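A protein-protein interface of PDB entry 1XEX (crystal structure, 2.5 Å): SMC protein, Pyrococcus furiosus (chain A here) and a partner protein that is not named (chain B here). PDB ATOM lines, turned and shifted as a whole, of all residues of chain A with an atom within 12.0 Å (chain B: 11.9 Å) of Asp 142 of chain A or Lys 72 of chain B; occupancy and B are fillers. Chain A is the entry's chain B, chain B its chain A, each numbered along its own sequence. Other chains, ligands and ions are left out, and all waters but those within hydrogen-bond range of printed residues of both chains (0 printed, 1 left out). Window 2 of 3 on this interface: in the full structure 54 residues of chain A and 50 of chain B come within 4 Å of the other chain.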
ATOM      1  N   VAL A 138     -10.539 -26.543  40.052  1.00  0.00           N
ATOM      2  CA  VAL A 138     -10.136 -25.896  38.815  1.00  0.00           C
ATOM      3  C   VAL A 138      -9.623 -24.510  39.159  1.00  0.00           C
ATOM      4  O   VAL A 138     -10.093 -23.899  40.106  1.00  0.00           O
ATOM      5  CB  VAL A 138     -11.327 -25.741  37.856  1.00  0.00           C
ATOM      6  CG1 VAL A 138     -10.862 -25.129  36.536  1.00  0.00           C
ATOM      7  CG2 VAL A 138     -12.018 -27.100  37.655  1.00  0.00           C
ATOM      8  N   SER A 139      -8.629 -24.027  38.419  1.00  0.00           N
ATOM      9  CA  SER A 139      -8.090 -22.686  38.655  1.00  0.00           C
ATOM     10  C   SER A 139      -7.521 -22.167  37.363  1.00  0.00           C
ATOM     11  O   SER A 139      -7.277 -22.922  36.428  1.00  0.00           O
ATOM     12  CB  SER A 139      -7.025 -22.668  39.762  1.00  0.00           C
ATOM     13  OG  SER A 139      -5.868 -23.395  39.423  1.00  0.00           O
ATOM     14  N   MET A 140      -7.329 -20.866  37.293  1.00  0.00           N
ATOM     15  CA  MET A 140      -6.828 -20.284  36.073  1.00  0.00           C
ATOM     16  C   MET A 140      -5.709 -19.310  36.346  1.00  0.00           C
ATOM     17  O   MET A 140      -5.703 -18.584  37.350  1.00  0.00           O
ATOM     18  CB  MET A 140      -7.957 -19.586  35.328  1.00  0.00           C
ATOM     19  CG  MET A 140      -7.558 -19.059  33.979  1.00  0.00           C
ATOM     20  SD  MET A 140      -8.922 -18.215  33.164  1.00  0.00           S
ATOM     21  CE  MET A 140      -9.617 -19.557  32.211  1.00  0.00           C
ATOM     22  N   ARG A 141      -4.747 -19.325  35.436  1.00  0.00           N
ATOM     23  CA  ARG A 141      -3.582 -18.478  35.523  1.00  0.00           C
ATOM     24  C   ARG A 141      -3.282 -17.994  34.111  1.00  0.00           C
ATOM     25  O   ARG A 141      -3.098 -18.794  33.187  1.00  0.00           O
ATOM     26  CB  ARG A 141      -2.410 -19.280  36.083  1.00  0.00           C
ATOM     27  CG  ARG A 141      -1.240 -18.418  36.470  1.00  0.00           C
ATOM     28  CD  ARG A 141      -0.093 -19.234  37.010  1.00  0.00           C
ATOM     29  NE  ARG A 141       1.064 -18.380  37.247  1.00  0.00           N
ATOM     30  CZ  ARG A 141       2.262 -18.822  37.611  1.00  0.00           C
ATOM     31  NH1 ARG A 141       3.249 -17.953  37.795  1.00  0.00           N
ATOM     32  NH2 ARG A 141       2.470 -20.123  37.786  1.00  0.00           N
ATOM     33  N   ASP A 142      -3.268 -16.682  33.943  1.00  0.00           N
ATOM     34  CA  ASP A 142      -3.005 -16.104  32.637  1.00  0.00           C
ATOM     35  C   ASP A 142      -3.882 -16.731  31.540  1.00  0.00           C
ATOM     36  O   ASP A 142      -3.393 -17.170  30.489  1.00  0.00           O
ATOM     37  CB  ASP A 142      -1.510 -16.238  32.302  1.00  0.00           C
ATOM     38  CG  ASP A 142      -0.622 -15.446  33.268  1.00  0.00           C
ATOM     39  OD1 ASP A 142       0.278 -16.052  33.900  1.00  0.00           O
ATOM     40  OD2 ASP A 142      -0.830 -14.217  33.397  1.00  0.00           O
ATOM     41  N   GLY A 143      -5.185 -16.775  31.802  1.00  0.00           N
ATOM     42  CA  GLY A 143      -6.126 -17.306  30.835  1.00  0.00           C
ATOM     43  C   GLY A 143      -6.088 -18.796  30.574  1.00  0.00           C
ATOM     44  O   GLY A 143      -6.787 -19.263  29.678  1.00  0.00           O
ATOM     45  N   VAL A 144      -5.302 -19.549  31.347  1.00  0.00           N
ATOM     46  CA  VAL A 144      -5.211 -20.994  31.136  1.00  0.00           C
ATOM     47  C   VAL A 144      -5.784 -21.810  32.302  1.00  0.00           C
ATOM     48  O   VAL A 144      -5.366 -21.647  33.440  1.00  0.00           O
ATOM     49  CB  VAL A 144      -3.737 -21.426  30.914  1.00  0.00           C
ATOM     50  CG1 VAL A 144      -3.672 -22.892  30.483  1.00  0.00           C
ATOM     51  CG2 VAL A 144      -3.093 -20.534  29.865  1.00  0.00           C
ATOM     52  N   SER A 145      -6.721 -22.705  32.011  1.00  0.00           N
ATOM     53  CA  SER A 145      -7.316 -23.519  33.060  1.00  0.00           C
ATOM     54  C   SER A 145      -6.410 -24.666  33.458  1.00  0.00           C
ATOM     55  O   SER A 145      -5.775 -25.299  32.611  1.00  0.00           O
ATOM     56  CB  SER A 145      -8.673 -24.101  32.622  1.00  0.00           C
ATOM     57  OG  SER A 145      -9.628 -23.095  32.459  1.00  0.00           O
ATOM     58  N   LYS A 146      -6.383 -24.935  34.757  1.00  0.00           N
ATOM     59  CA  LYS A 146      -5.586 -26.013  35.300  1.00  0.00           C
ATOM     60  C   LYS A 146      -6.441 -26.829  36.282  1.00  0.00           C
ATOM     61  O   LYS A 146      -7.417 -26.320  36.852  1.00  0.00           O
ATOM     62  CB  LYS A 146      -4.350 -25.439  35.985  1.00  0.00           C
ATOM     63  CG  LYS A 146      -3.251 -26.451  36.239  1.00  0.00           C
ATOM     64  CD  LYS A 146      -1.976 -25.721  36.645  1.00  0.00           C
ATOM     65  CE  LYS A 146      -0.835 -26.668  36.948  1.00  0.00           C
ATOM     66  NZ  LYS A 146       0.453 -25.902  37.042  1.00  0.00           N
ATOM     67  N   LYS B  13     -11.307 -25.027  24.557  1.00  0.00           N
ATOM     68  CA  LYS B  13     -11.740 -23.825  25.273  1.00  0.00           C
ATOM     69  C   LYS B  13     -10.630 -23.261  26.167  1.00  0.00           C
ATOM     70  O   LYS B  13      -9.549 -22.996  25.668  1.00  0.00           O
ATOM     71  CB  LYS B  13     -13.036 -24.104  26.048  1.00  0.00           C
ATOM     72  CG  LYS B  13     -14.147 -24.582  25.106  1.00  0.00           C
ATOM     73  CD  LYS B  13     -15.538 -24.619  25.736  1.00  0.00           C
ATOM     74  CE  LYS B  13     -16.032 -23.230  26.055  1.00  0.00           C
ATOM     75  NZ  LYS B  13     -17.495 -23.220  26.319  1.00  0.00           N
ATOM     76  N   SER B  14     -10.863 -23.083  27.462  1.00  0.00           N
ATOM     77  CA  SER B  14      -9.818 -22.498  28.317  1.00  0.00           C
ATOM     78  C   SER B  14      -8.619 -23.386  28.657  1.00  0.00           C
ATOM     79  O   SER B  14      -7.715 -22.944  29.369  1.00  0.00           O
ATOM     80  CB  SER B  14     -10.409 -21.986  29.634  1.00  0.00           C
ATOM     81  OG  SER B  14     -10.933 -23.052  30.410  1.00  0.00           O
ATOM     82  N   TYR B  15      -8.609 -24.622  28.178  1.00  0.00           N
ATOM     83  CA  TYR B  15      -7.493 -25.505  28.464  1.00  0.00           C
ATOM     84  C   TYR B  15      -6.463 -25.349  27.339  1.00  0.00           C
ATOM     85  O   TYR B  15      -6.746 -25.644  26.164  1.00  0.00           O
ATOM     86  CB  TYR B  15      -8.001 -26.949  28.614  1.00  0.00           C
ATOM     87  CG  TYR B  15      -8.870 -27.096  29.841  1.00  0.00           C
ATOM     88  CD1 TYR B  15      -8.322 -27.454  31.080  1.00  0.00           C
ATOM     89  CD2 TYR B  15     -10.219 -26.721  29.803  1.00  0.00           C
ATOM     90  CE1 TYR B  15      -9.097 -27.421  32.261  1.00  0.00           C
ATOM     91  CE2 TYR B  15     -11.006 -26.676  30.971  1.00  0.00           C
ATOM     92  CZ  TYR B  15     -10.443 -27.024  32.195  1.00  0.00           C
ATOM     93  OH  TYR B  15     -11.217 -26.929  33.331  1.00  0.00           O
ATOM     94  N   GLY B  16      -5.281 -24.854  27.711  1.00  0.00           N
ATOM     95  CA  GLY B  16      -4.206 -24.599  26.759  1.00  0.00           C
ATOM     96  C   GLY B  16      -3.742 -25.723  25.850  1.00  0.00           C
ATOM     97  O   GLY B  16      -4.475 -26.671  25.615  1.00  0.00           O
ATOM     98  N   ASN B  17      -2.522 -25.603  25.325  1.00  0.00           N
ATOM     99  CA  ASN B  17      -1.954 -26.601  24.411  1.00  0.00           C
ATOM    100  C   ASN B  17      -1.322 -27.770  25.144  1.00  0.00           C
ATOM    101  O   ASN B  17      -1.154 -28.849  24.577  1.00  0.00           O
ATOM    102  CB  ASN B  17      -0.904 -25.963  23.494  1.00  0.00           C
ATOM    103  CG  ASN B  17      -1.505 -24.957  22.526  1.00  0.00           C
ATOM    104  OD1 ASN B  17      -1.318 -23.752  22.675  1.00  0.00           O
ATOM    105  ND2 ASN B  17      -2.236 -25.451  21.526  1.00  0.00           N
ATOM    106  N   LYS B  18      -0.958 -27.532  26.398  1.00  0.00           N
ATOM    107  CA  LYS B  18      -0.355 -28.544  27.256  1.00  0.00           C
ATOM    108  C   LYS B  18      -1.491 -29.441  27.743  1.00  0.00           C
ATOM    109  O   LYS B  18      -2.227 -29.080  28.654  1.00  0.00           O
ATOM    110  CB  LYS B  18       0.335 -27.850  28.436  1.00  0.00           C
ATOM    111  CG  LYS B  18       0.825 -28.764  29.545  1.00  0.00           C
ATOM    112  N   ALA B  34     -12.852 -21.108  41.407  1.00  0.00           N
ATOM    113  CA  ALA B  34     -13.276 -19.715  41.317  1.00  0.00           C
ATOM    114  C   ALA B  34     -14.188 -19.503  40.115  1.00  0.00           C
ATOM    115  O   ALA B  34     -14.159 -20.293  39.157  1.00  0.00           O
ATOM    116  CB  ALA B  34     -12.044 -18.794  41.190  1.00  0.00           C
ATOM    117  N   ASN B  35     -15.002 -18.448  40.161  1.00  0.00           N
ATOM    118  CA  ASN B  35     -15.869 -18.139  39.022  1.00  0.00           C
ATOM    119  C   ASN B  35     -14.956 -17.826  37.817  1.00  0.00           C
ATOM    120  O   ASN B  35     -13.934 -17.112  37.954  1.00  0.00           O
ATOM    121  CB  ASN B  35     -16.741 -16.904  39.315  1.00  0.00           C
ATOM    122  CG  ASN B  35     -17.864 -17.180  40.314  1.00  0.00           C
ATOM    123  OD1 ASN B  35     -18.078 -16.402  41.244  1.00  0.00           O
ATOM    124  ND2 ASN B  35     -18.606 -18.267  40.099  1.00  0.00           N
ATOM    125  N   GLY B  36     -15.336 -18.348  36.651  1.00  0.00           N
ATOM    126  CA  GLY B  36     -14.590 -18.121  35.413  1.00  0.00           C
ATOM    127  C   GLY B  36     -13.264 -18.860  35.280  1.00  0.00           C
ATOM    128  O   GLY B  36     -12.404 -18.445  34.491  1.00  0.00           O
ATOM    129  N   SER B  37     -13.088 -19.942  36.039  1.00  0.00           N
ATOM    130  CA  SER B  37     -11.846 -20.698  36.014  1.00  0.00           C
ATOM    131  C   SER B  37     -11.853 -21.832  35.010  1.00  0.00           C
ATOM    132  O   SER B  37     -10.794 -22.285  34.600  1.00  0.00           O
ATOM    133  CB  SER B  37     -11.497 -21.253  37.409  1.00  0.00           C
ATOM    134  OG  SER B  37     -12.480 -22.156  37.912  1.00  0.00           O
ATOM    135  N   GLY B  38     -13.033 -22.287  34.609  1.00  0.00           N
ATOM    136  CA  GLY B  38     -13.086 -23.367  33.645  1.00  0.00           C
ATOM    137  C   GLY B  38     -13.830 -24.618  34.090  1.00  0.00           C
ATOM    138  O   GLY B  38     -13.630 -25.684  33.521  1.00  0.00           O
ATOM    139  N   ASN B  41     -16.557 -25.536  31.403  1.00  0.00           N
ATOM    140  CA  ASN B  41     -15.891 -25.964  30.182  1.00  0.00           C
ATOM    141  C   ASN B  41     -15.620 -27.473  30.197  1.00  0.00           C
ATOM    142  O   ASN B  41     -15.560 -28.120  29.134  1.00  0.00           O
ATOM    143  CB  ASN B  41     -14.579 -25.205  29.983  1.00  0.00           C
ATOM    144  CG  ASN B  41     -14.795 -23.734  29.677  1.00  0.00           C
ATOM    145  OD1 ASN B  41     -15.907 -23.308  29.356  1.00  0.00           O
ATOM    146  ND2 ASN B  41     -13.724 -22.947  29.773  1.00  0.00           N
ATOM    147  N   PHE B  68      -8.942 -23.251  21.640  1.00  0.00           N
ATOM    148  CA  PHE B  68      -8.220 -22.388  22.564  1.00  0.00           C
ATOM    149  C   PHE B  68      -7.701 -21.086  21.956  1.00  0.00           C
ATOM    150  O   PHE B  68      -6.924 -21.098  21.007  1.00  0.00           O
ATOM    151  CB  PHE B  68      -7.059 -23.159  23.173  1.00  0.00           C
ATOM    152  CG  PHE B  68      -6.168 -22.319  24.045  1.00  0.00           C
ATOM    153  CD1 PHE B  68      -6.632 -21.830  25.268  1.00  0.00           C
ATOM    154  CD2 PHE B  68      -4.869 -22.012  23.640  1.00  0.00           C
ATOM    155  CE1 PHE B  68      -5.815 -21.050  26.072  1.00  0.00           C
ATOM    156  CE2 PHE B  68      -4.042 -21.233  24.433  1.00  0.00           C
ATOM    157  CZ  PHE B  68      -4.508 -20.746  25.654  1.00  0.00           C
ATOM    158  N   ALA B  69      -8.119 -19.970  22.543  1.00  0.00           N
ATOM    159  CA  ALA B  69      -7.740 -18.637  22.087  1.00  0.00           C
ATOM    160  C   ALA B  69      -6.429 -18.162  22.683  1.00  0.00           C
ATOM    161  O   ALA B  69      -6.265 -18.114  23.904  1.00  0.00           O
ATOM    162  CB  ALA B  69      -8.839 -17.639  22.427  1.00  0.00           C
ATOM    163  N   GLY B  70      -5.500 -17.795  21.805  1.00  0.00           N
ATOM    164  CA  GLY B  70      -4.203 -17.318  22.248  1.00  0.00           C
ATOM    165  C   GLY B  70      -4.282 -16.476  23.508  1.00  0.00           C
ATOM    166  O   GLY B  70      -5.171 -15.637  23.666  1.00  0.00           O
ATOM    167  N   SER B  71      -3.333 -16.707  24.405  1.00  0.00           N
ATOM    168  CA  SER B  71      -3.274 -15.998  25.670  1.00  0.00           C
ATOM    169  C   SER B  71      -1.967 -15.210  25.841  1.00  0.00           C
ATOM    170  O   SER B  71      -1.259 -14.927  24.863  1.00  0.00           O
ATOM    171  CB  SER B  71      -3.430 -17.001  26.818  1.00  0.00           C
ATOM    172  OG  SER B  71      -2.487 -18.057  26.686  1.00  0.00           O
ATOM    173  N   LYS B  72      -1.660 -14.867  27.092  1.00  0.00           N
ATOM    174  CA  LYS B  72      -0.458 -14.113  27.415  1.00  0.00           C
ATOM    175  C   LYS B  72       0.775 -14.809  26.859  1.00  0.00           C
ATOM    176  O   LYS B  72       1.304 -14.417  25.811  1.00  0.00           O
ATOM    177  CB  LYS B  72      -0.327 -13.939  28.937  1.00  0.00           C
ATOM    178  CG  LYS B  72       0.912 -13.154  29.361  1.00  0.00           C
ATOM    179  CD  LYS B  72       0.779 -12.576  30.763  1.00  0.00           C
ATOM    180  CE  LYS B  72       1.976 -11.688  31.100  1.00  0.00           C
ATOM    181  NZ  LYS B  72       1.705 -10.729  32.217  1.00  0.00           N
ATOM    182  N   ASN B  73       1.226 -15.845  27.558  1.00  0.00           N
ATOM    183  CA  ASN B  73       2.399 -16.595  27.131  1.00  0.00           C
ATOM    184  C   ASN B  73       2.014 -17.925  26.479  1.00  0.00           C
ATOM    185  O   ASN B  73       2.460 -18.991  26.920  1.00  0.00           O
ATOM    186  CB  ASN B  73       3.326 -16.847  28.328  1.00  0.00           C
ATOM    187  CG  ASN B  73       2.594 -16.783  29.662  1.00  0.00           C
ATOM    188  OD1 ASN B  73       2.319 -15.699  30.179  1.00  0.00           O
ATOM    189  ND2 ASN B  73       2.267 -17.947  30.218  1.00  0.00           N
ATOM    190  N   GLU B  74       1.201 -17.859  25.423  1.00  0.00           N
ATOM    191  CA  GLU B  74       0.756 -19.065  24.724  1.00  0.00           C
ATOM    192  C   GLU B  74      -0.033 -18.778  23.433  1.00  0.00           C
ATOM    193  O   GLU B  74      -0.974 -17.981  23.431  1.00  0.00           O
ATOM    194  CB  GLU B  74      -0.087 -19.910  25.685  1.00  0.00           C
ATOM    195  CG  GLU B  74      -0.570 -21.233  25.137  1.00  0.00           C
ATOM    196  CD  GLU B  74      -0.738 -22.271  26.232  1.00  0.00           C
ATOM    197  OE1 GLU B  74      -1.382 -23.314  25.980  1.00  0.00           O
ATOM    198  OE2 GLU B  74      -0.213 -22.048  27.348  1.00  0.00           O
ATOM    199  N   PRO B  75       0.363 -19.415  22.315  1.00  0.00           N
ATOM    200  CA  PRO B  75      -0.293 -19.245  21.010  1.00  0.00           C
ATOM    201  C   PRO B  75      -1.618 -19.999  20.934  1.00  0.00           C
ATOM    202  O   PRO B  75      -1.880 -20.898  21.729  1.00  0.00           O
ATOM    203  CB  PRO B  75       0.726 -19.817  20.022  1.00  0.00           C
ATOM    204  CG  PRO B  75       2.031 -19.690  20.747  1.00  0.00           C
ATOM    205  CD  PRO B  75       1.657 -20.096  22.149  1.00  0.00           C
ATOM    206  N   PRO B  76      -2.469 -19.645  19.963  1.00  0.00           N
ATOM    207  CA  PRO B  76      -3.758 -20.326  19.829  1.00  0.00           C
ATOM    208  C   PRO B  76      -3.553 -21.759  19.347  1.00  0.00           C
ATOM    209  O   PRO B  76      -2.553 -22.070  18.689  1.00  0.00           O
ATOM    210  CB  PRO B  76      -4.499 -19.462  18.810  1.00  0.00           C
ATOM    211  CG  PRO B  76      -3.391 -19.004  17.911  1.00  0.00           C
ATOM    212  CD  PRO B  76      -2.289 -18.639  18.898  1.00  0.00           C
ATOM    213  N   ALA B  77      -4.503 -22.627  19.681  1.00  0.00           N
ATOM    214  CA  ALA B  77      -4.435 -24.031  19.290  1.00  0.00           C
ATOM    215  C   ALA B  77      -4.620 -24.177  17.790  1.00  0.00           C
ATOM    216  O   ALA B  77      -5.243 -23.336  17.153  1.00  0.00           O
ATOM    217  CB  ALA B  77      -5.517 -24.821  20.016  1.00  0.00           C
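The side-chain hydroxyl (OH) of Tyr 15 of chain B sits at hydrogen-bond distance from the backbone carbonyl oxygen (O) of Gly 38 of chain B.
N of Lys 146 of chain A is in hydrogen-bond range of O of Ser 139 of chain A (2.8 Å).
The side-chain hydroxyl of Ser 14 of chain B is in hydrogen-bond range of the side-chain amide nitrogen of Asn 41 of chain B (2.9 Å).
The backbone carbonyl oxygen (O) of Ala 34 of chain B lies within hydrogen-bond range of the side-chain hydroxyl (OG) of Ser 37 of chain B (2.8 Å).
Of the printed residues of chain B, Val 138 of chain A touches Tyr 15 (3.7 Å), Ser 37 (3.4 Å) and Gly 38 (3.9 Å).
Printed residues of chain B within 4 Å of Ser 139 of chain A: Ser 37.
No residue of chain B comes within 4 Å of Arg 141 of chain A.
Of chain B, only Ser 71 and Lys 72 come within 4 Å of Asp 142 of chain A.
Printed residues of chain B within 4 Å of Val 144 of chain A: Ser 14 (3.6 Å) and Gly 16 (3.8 Å).
Printed residues of chain B within 4 Å of Ser 145 of chain A: Ser 14 (2.4 Å), Tyr 15 (3.4 Å), Ser 37 (2.6 Å) and Gly 38 (3.7 Å).
Of the printed residues of chain A, Tyr 15 of chain B touches Val 138 (3.7 Å) and Ser 145 (3.4 Å).
Printed residues of chain A within 4 Å of Gly 38 of chain B: Val 138 and Ser 145.
Asn 41 of chain B touches none of the printed residues of chain A.
No residue of chain A comes within 4 Å of Gly 70 of chain B.
Of the printed residues of chain A, Lys 72 of chain B touches Asp 142.
No residue of chain A comes within 4 Å of Asn 73 of chain B.
No residue of chain A comes within 4 Å of Glu 74 of chain B.
Pro 75 of chain B touches none of the printed residues of chain A.
Among the printed residues, merely in contact across the chains: Ser 145 of chain A with Tyr 15 of chain B (3.4 Å), Val 138 of chain A with Ser 37 of chain B (3.4 Å), Asp 142 of chain A with Lys 72 of chain B (3.5 Å), Met 140 of chain A with Ser 14 of chain B (3.6 Å), Val 144 of chain A with Ser 14 of chain B (3.6 Å), Ser 145 of chain A with Gly 38 of chain B (3.7 Å), Asp 142 of chain A with Ser 71 of chain B (3.7 Å), Val 138 of chain A with Tyr 15 of chain B (3.7 Å), Val 144 of chain A with Gly 16 of chain B (3.8 Å), Gly 143 of chain A with Ser 14 of chain B (3.8 Å), Met 140 of chain A with Ser 37 of chain B (3.8 Å), Val 138 of chain A with Gly 38 of chain B (3.9 Å) and Ser 139 of chain A with Ser 37 of chain B (3.9 Å).
The side-chain sulfur (SD) of Met 140 of chain A sits close to the backbone carbonyl oxygen (O) of Gly 36 of chain B (3.7 Å).
OG of Ser 14 of chain B sits at hydrogen-bond distance from OG of Ser 145 of chain A, 2.4 Å away.
OG of Ser 145 of chain A lies within hydrogen-bond range of O of Ser 37 of chain B.
Of the 9 printed residues of chain A, 7 touch a printed residue of chain B.
Hydrophobic or aromatic side chains of chain A within 4 Å of the printed part of chain B: Val 138, Met 140 and Val 144.
Of the 22 printed residues of chain B, 8 touch a printed residue of chain A.
Hydrophobic or aromatic side chains of chain B within 4 Å of the printed part of chain A: Tyr 15.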
